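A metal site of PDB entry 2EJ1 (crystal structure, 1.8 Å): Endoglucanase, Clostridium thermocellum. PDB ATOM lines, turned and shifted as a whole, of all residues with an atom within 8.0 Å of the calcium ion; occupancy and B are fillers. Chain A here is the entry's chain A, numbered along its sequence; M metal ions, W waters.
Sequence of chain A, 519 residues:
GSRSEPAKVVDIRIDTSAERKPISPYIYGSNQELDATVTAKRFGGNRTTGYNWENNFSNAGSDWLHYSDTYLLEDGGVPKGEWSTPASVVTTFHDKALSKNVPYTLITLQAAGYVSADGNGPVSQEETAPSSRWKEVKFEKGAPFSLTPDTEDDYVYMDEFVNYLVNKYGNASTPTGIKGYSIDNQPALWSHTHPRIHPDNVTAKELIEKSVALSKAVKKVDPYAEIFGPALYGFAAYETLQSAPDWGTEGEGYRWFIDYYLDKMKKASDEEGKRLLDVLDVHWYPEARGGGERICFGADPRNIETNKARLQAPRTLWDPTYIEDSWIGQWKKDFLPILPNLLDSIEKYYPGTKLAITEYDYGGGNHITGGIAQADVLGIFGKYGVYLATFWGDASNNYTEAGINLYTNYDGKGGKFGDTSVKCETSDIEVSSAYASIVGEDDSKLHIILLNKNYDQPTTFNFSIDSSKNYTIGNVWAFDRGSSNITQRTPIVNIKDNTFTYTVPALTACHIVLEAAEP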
ATOM      1  N   ASN A  52      14.421  23.291  12.375  1.00  0.00           N
ATOM      2  CA  ASN A  52      14.891  22.847  11.065  1.00  0.00           C
ATOM      3  C   ASN A  52      16.167  22.033  11.265  1.00  0.00           C
ATOM      4  O   ASN A  52      17.223  22.581  11.559  1.00  0.00           O
ATOM      5  CB  ASN A  52      15.160  24.074  10.179  1.00  0.00           C
ATOM      6  CG  ASN A  52      15.545  23.728   8.758  1.00  0.00           C
ATOM      7  OD1 ASN A  52      15.469  24.570   7.858  1.00  0.00           O
ATOM      8  ND2 ASN A  52      15.965  22.490   8.541  1.00  0.00           N
ATOM      9  N   TRP A  53      16.066  20.708  11.113  1.00  0.00           N
ATOM     10  CA  TRP A  53      17.225  19.853  11.322  1.00  0.00           C
ATOM     11  C   TRP A  53      18.368  20.084  10.351  1.00  0.00           C
ATOM     12  O   TRP A  53      19.523  19.746  10.655  1.00  0.00           O
ATOM     13  CB  TRP A  53      16.800  18.371  11.265  1.00  0.00           C
ATOM     14  CG  TRP A  53      16.652  17.812   9.872  1.00  0.00           C
ATOM     15  CD1 TRP A  53      15.599  18.006   9.018  1.00  0.00           C
ATOM     16  CD2 TRP A  53      17.599  16.997   9.173  1.00  0.00           C
ATOM     17  NE1 TRP A  53      15.841  17.349   7.824  1.00  0.00           N
ATOM     18  CE2 TRP A  53      17.051  16.726   7.896  1.00  0.00           C
ATOM     19  CE3 TRP A  53      18.843  16.465   9.512  1.00  0.00           C
ATOM     20  CZ2 TRP A  53      17.723  15.944   6.952  1.00  0.00           C
ATOM     21  CZ3 TRP A  53      19.515  15.682   8.568  1.00  0.00           C
ATOM     22  CH2 TRP A  53      18.952  15.428   7.308  1.00  0.00           C
ATOM     23  N   GLU A  54      18.087  20.672   9.198  1.00  0.00           N
ATOM     24  CA  GLU A  54      19.135  20.910   8.208  1.00  0.00           C
ATOM     25  C   GLU A  54      20.151  21.945   8.665  1.00  0.00           C
ATOM     26  O   GLU A  54      21.341  21.825   8.368  1.00  0.00           O
ATOM     27  CB  GLU A  54      18.523  21.356   6.872  1.00  0.00           C
ATOM     28  CG  GLU A  54      17.453  20.416   6.322  1.00  0.00           C
ATOM     29  CD  GLU A  54      17.083  20.712   4.877  1.00  0.00           C
ATOM     30  OE1 GLU A  54      17.218  21.884   4.452  1.00  0.00           O
ATOM     31  OE2 GLU A  54      16.650  19.794   4.158  1.00  0.00           O
ATOM     32  N   ASN A  55      19.695  22.959   9.407  1.00  0.00           N
ATOM     33  CA  ASN A  55      20.590  24.018   9.875  1.00  0.00           C
ATOM     34  C   ASN A  55      20.477  24.363  11.358  1.00  0.00           C
ATOM     35  O   ASN A  55      21.175  25.251  11.847  1.00  0.00           O
ATOM     36  CB  ASN A  55      20.367  25.274   9.037  1.00  0.00           C
ATOM     37  CG  ASN A  55      18.909  25.684   8.982  1.00  0.00           C
ATOM     38  OD1 ASN A  55      18.175  25.487   9.947  1.00  0.00           O
ATOM     39  ND2 ASN A  55      18.488  26.251   7.855  1.00  0.00           N
ATOM     40  N   VAL A 115       9.380  25.177   8.890  1.00  0.00           N
ATOM     41  CA  VAL A 115      10.461  25.277   9.865  1.00  0.00           C
ATOM     42  C   VAL A 115      11.331  26.481   9.473  1.00  0.00           C
ATOM     43  O   VAL A 115      11.345  26.894   8.315  1.00  0.00           O
ATOM     44  CB  VAL A 115      11.311  23.987   9.941  1.00  0.00           C
ATOM     45  CG1 VAL A 115      10.438  22.831  10.411  1.00  0.00           C
ATOM     46  CG2 VAL A 115      11.916  23.673   8.574  1.00  0.00           C
ATOM     47  N   LYS A 135      10.818  27.171   5.370  1.00  0.00           N
ATOM     48  CA  LYS A 135      10.999  26.049   4.463  1.00  0.00           C
ATOM     49  C   LYS A 135       9.797  25.150   4.734  1.00  0.00           C
ATOM     50  O   LYS A 135       9.428  24.924   5.891  1.00  0.00           O
ATOM     51  CB  LYS A 135      12.292  25.279   4.774  1.00  0.00           C
ATOM     52  CG  LYS A 135      13.582  26.055   4.512  1.00  0.00           C
ATOM     53  CD  LYS A 135      13.655  26.537   3.070  1.00  0.00           C
ATOM     54  CE  LYS A 135      15.018  27.179   2.783  1.00  0.00           C
ATOM     55  NZ  LYS A 135      15.088  27.757   1.418  1.00  0.00           N
ATOM     56  N   GLU A 136       9.176  24.653   3.673  1.00  0.00           N
ATOM     57  CA  GLU A 136       8.015  23.792   3.827  1.00  0.00           C
ATOM     58  C   GLU A 136       8.448  22.398   4.251  1.00  0.00           C
ATOM     59  O   GLU A 136       9.413  21.854   3.732  1.00  0.00           O
ATOM     60  CB  GLU A 136       7.245  23.687   2.511  1.00  0.00           C
ATOM     61  CG  GLU A 136       5.923  22.930   2.611  1.00  0.00           C
ATOM     62  CD  GLU A 136       5.244  22.754   1.267  1.00  0.00           C
ATOM     63  OE1 GLU A 136       5.287  23.697   0.441  1.00  0.00           O
ATOM     64  OE2 GLU A 136       4.655  21.683   1.039  1.00  0.00           O
ATOM     65  N   LYS A 141      10.499  12.296   1.510  1.00  0.00           N
ATOM     66  CA  LYS A 141      11.271  12.918   0.429  1.00  0.00           C
ATOM     67  C   LYS A 141      10.894  12.363  -0.944  1.00  0.00           C
ATOM     68  O   LYS A 141      10.774  13.125  -1.909  1.00  0.00           O
ATOM     69  CB  LYS A 141      12.762  12.719   0.679  1.00  0.00           C
ATOM     70  CG  LYS A 141      13.645  13.551  -0.255  1.00  0.00           C
ATOM     71  CD  LYS A 141      15.120  13.365   0.048  1.00  0.00           C
ATOM     72  CE  LYS A 141      15.961  14.306  -0.796  1.00  0.00           C
ATOM     73  NZ  LYS A 141      17.417  14.097  -0.591  1.00  0.00           N
ATOM     74  N   THR A 148      23.793  14.884   3.849  1.00  0.00           N
ATOM     75  CA  THR A 148      24.149  16.299   3.737  1.00  0.00           C
ATOM     76  C   THR A 148      22.985  16.991   3.032  1.00  0.00           C
ATOM     77  O   THR A 148      23.088  17.384   1.867  1.00  0.00           O
ATOM     78  CB  THR A 148      25.453  16.507   2.939  1.00  0.00           C
ATOM     79  OG1 THR A 148      25.339  15.882   1.651  1.00  0.00           O
ATOM     80  CG2 THR A 148      26.629  15.918   3.681  1.00  0.00           C
ATOM     81  N   PRO A 149      21.861  17.161   3.745  1.00  0.00           N
ATOM     82  CA  PRO A 149      20.659  17.802   3.220  1.00  0.00           C
ATOM     83  C   PRO A 149      20.898  19.145   2.531  1.00  0.00           C
ATOM     84  O   PRO A 149      21.703  19.951   2.984  1.00  0.00           O
ATOM     85  CB  PRO A 149      19.748  17.910   4.442  1.00  0.00           C
ATOM     86  CG  PRO A 149      20.727  18.035   5.571  1.00  0.00           C
ATOM     87  CD  PRO A 149      21.746  16.981   5.203  1.00  0.00           C
ATOM     88  N   ASP A 150      20.165  19.358   1.448  1.00  0.00           N
ATOM     89  CA  ASP A 150      20.253  20.575   0.659  1.00  0.00           C
ATOM     90  C   ASP A 150      19.522  21.706   1.385  1.00  0.00           C
ATOM     91  O   ASP A 150      18.296  21.684   1.476  1.00  0.00           O
ATOM     92  CB  ASP A 150      19.614  20.342  -0.710  1.00  0.00           C
ATOM     93  CG  ASP A 150      19.782  21.510  -1.648  1.00  0.00           C
ATOM     94  OD1 ASP A 150      20.198  22.600  -1.204  1.00  0.00           O
ATOM     95  OD2 ASP A 150      19.472  21.336  -2.850  1.00  0.00           O
ATOM     96  N   THR A 151      20.276  22.673   1.904  1.00  0.00           N
ATOM     97  CA  THR A 151      19.680  23.788   2.624  1.00  0.00           C
ATOM     98  C   THR A 151      19.230  24.896   1.676  1.00  0.00           C
ATOM     99  O   THR A 151      18.656  25.896   2.109  1.00  0.00           O
ATOM    100  CB  THR A 151      20.666  24.391   3.640  1.00  0.00           C
ATOM    101  OG1 THR A 151      21.837  24.852   2.958  1.00  0.00           O
ATOM    102  CG2 THR A 151      21.064  23.347   4.679  1.00  0.00           C
ATOM    103  N   GLU A 152      19.473  24.705   0.387  1.00  0.00           N
ATOM    104  CA  GLU A 152      19.118  25.702  -0.614  1.00  0.00           C
ATOM    105  C   GLU A 152      17.726  25.539  -1.237  1.00  0.00           C
ATOM    106  O   GLU A 152      17.160  26.505  -1.752  1.00  0.00           O
ATOM    107  CB  GLU A 152      20.157  25.715  -1.740  1.00  0.00           C
ATOM    108  CG  GLU A 152      21.592  25.846  -1.246  1.00  0.00           C
ATOM    109  CD  GLU A 152      21.807  27.071  -0.388  1.00  0.00           C
ATOM    110  OE1 GLU A 152      21.638  28.194  -0.899  1.00  0.00           O
ATOM    111  OE2 GLU A 152      22.155  26.909   0.802  1.00  0.00           O
ATOM    112  N   ASP A 153      17.168  24.329  -1.209  1.00  0.00           N
ATOM    113  CA  ASP A 153      15.845  24.126  -1.780  1.00  0.00           C
ATOM    114  C   ASP A 153      14.780  24.615  -0.795  1.00  0.00           C
ATOM    115  O   ASP A 153      15.097  25.071   0.299  1.00  0.00           O
ATOM    116  CB  ASP A 153      15.611  22.659  -2.175  1.00  0.00           C
ATOM    117  CG  ASP A 153      15.710  21.711  -1.012  1.00  0.00           C
ATOM    118  OD1 ASP A 153      15.572  22.156   0.153  1.00  0.00           O
ATOM    119  OD2 ASP A 153      15.914  20.503  -1.259  1.00  0.00           O
ATOM    120  N   ASP A 154      13.506  24.508  -1.186  1.00  0.00           N
ATOM    121  CA  ASP A 154      12.435  25.001  -0.326  1.00  0.00           C
ATOM    122  C   ASP A 154      11.803  23.995   0.611  1.00  0.00           C
ATOM    123  O   ASP A 154      10.783  24.297   1.249  1.00  0.00           O
ATOM    124  CB  ASP A 154      11.333  25.628  -1.181  1.00  0.00           C
ATOM    125  CG  ASP A 154      11.856  26.632  -2.187  1.00  0.00           C
ATOM    126  OD1 ASP A 154      12.659  27.505  -1.789  1.00  0.00           O
ATOM    127  OD2 ASP A 154      11.465  26.548  -3.360  1.00  0.00           O
ATOM    128  N   TYR A 155      12.388  22.804   0.735  1.00  0.00           N
ATOM    129  CA  TYR A 155      11.801  21.770   1.576  1.00  0.00           C
ATOM    130  C   TYR A 155      12.726  21.149   2.621  1.00  0.00           C
ATOM    131  O   TYR A 155      13.944  21.124   2.464  1.00  0.00           O
ATOM    132  CB  TYR A 155      11.260  20.646   0.697  1.00  0.00           C
ATOM    133  CG  TYR A 155      10.237  21.097  -0.312  1.00  0.00           C
ATOM    134  CD1 TYR A 155       8.923  21.386   0.073  1.00  0.00           C
ATOM    135  CD2 TYR A 155      10.575  21.269  -1.652  1.00  0.00           C
ATOM    136  CE1 TYR A 155       7.981  21.828  -0.846  1.00  0.00           C
ATOM    137  CE2 TYR A 155       9.639  21.722  -2.588  1.00  0.00           C
ATOM    138  CZ  TYR A 155       8.339  21.996  -2.176  1.00  0.00           C
ATOM    139  OH  TYR A 155       7.406  22.433  -3.095  1.00  0.00           O
ATOM    140  N   VAL A 156      12.106  20.645   3.682  1.00  0.00           N
ATOM    141  CA  VAL A 156      12.811  19.950   4.749  1.00  0.00           C
ATOM    142  C   VAL A 156      12.018  18.661   4.906  1.00  0.00           C
ATOM    143  O   VAL A 156      10.801  18.687   5.085  1.00  0.00           O
ATOM    144  CB  VAL A 156      12.795  20.751   6.066  1.00  0.00           C
ATOM    145  CG1 VAL A 156      13.403  19.914   7.177  1.00  0.00           C
ATOM    146  CG2 VAL A 156      13.585  22.035   5.900  1.00  0.00           C
ATOM    147  N   TYR A 157      12.712  17.530   4.833  1.00  0.00           N
ATOM    148  CA  TYR A 157      12.083  16.210   4.894  1.00  0.00           C
ATOM    149  C   TYR A 157      12.238  15.497   6.225  1.00  0.00           C
ATOM    150  O   TYR A 157      13.338  15.341   6.733  1.00  0.00           O
ATOM    151  CB  TYR A 157      12.646  15.343   3.764  1.00  0.00           C
ATOM    152  CG  TYR A 157      12.478  15.978   2.395  1.00  0.00           C
ATOM    153  CD1 TYR A 157      11.247  15.978   1.752  1.00  0.00           C
ATOM    154  CD2 TYR A 157      13.539  16.636   1.773  1.00  0.00           C
ATOM    155  CE1 TYR A 157      11.075  16.609   0.522  1.00  0.00           C
ATOM    156  CE2 TYR A 157      13.372  17.279   0.547  1.00  0.00           C
ATOM    157  CZ  TYR A 157      12.132  17.260  -0.074  1.00  0.00           C
ATOM    158  OH  TYR A 157      11.941  17.899  -1.281  1.00  0.00           O
ATOM    159  N   GLU A 160      14.049  11.988   6.022  1.00  0.00           N
ATOM    160  CA  GLU A 160      15.480  12.145   5.768  1.00  0.00           C
ATOM    161  C   GLU A 160      16.148  12.467   7.099  1.00  0.00           C
ATOM    162  O   GLU A 160      17.281  12.026   7.379  1.00  0.00           O
ATOM    163  CB  GLU A 160      15.722  13.253   4.743  1.00  0.00           C
ATOM    164  CG  GLU A 160      17.190  13.434   4.345  1.00  0.00           C
ATOM    165  CD  GLU A 160      17.358  14.340   3.128  1.00  0.00           C
ATOM    166  OE1 GLU A 160      16.905  15.496   3.177  1.00  0.00           O
ATOM    167  OE2 GLU A 160      17.945  13.881   2.120  1.00  0.00           O
HETATM  168 CA    CA M   1      16.180  21.322   2.293  1.00  0.00          CA
HETATM  169  O   HOH W   1      16.235  19.253   1.030  1.00  0.00           O
HETATM  170  O   HOH W   2      15.746  23.668   2.520  1.00  0.00           O
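The side-chain carboxylate of Asp 150 is in hydrogen-bond range of the backbone NH of Glu 152. The backbone NH (N) of Glu 54 lies close to the side-chain amide nitrogen (ND2) of Asn 52 (2.9 Å). The backbone carbonyl oxygen of Asp 153 is in hydrogen-bond range of the side-chain amino group of Lys 135, 2.9 Å away.
The nearest printed residue that does not touch the calcium ion is Thr 151 (4.3 Å).
The calcium ion is bound by O of Tyr 155, O of Asp 150, OD1 of Asp 153, water W2, water W1, OE2 of Glu 54 and OE1 of Glu 54. The calcium ion has seven donor atoms within binding distance.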
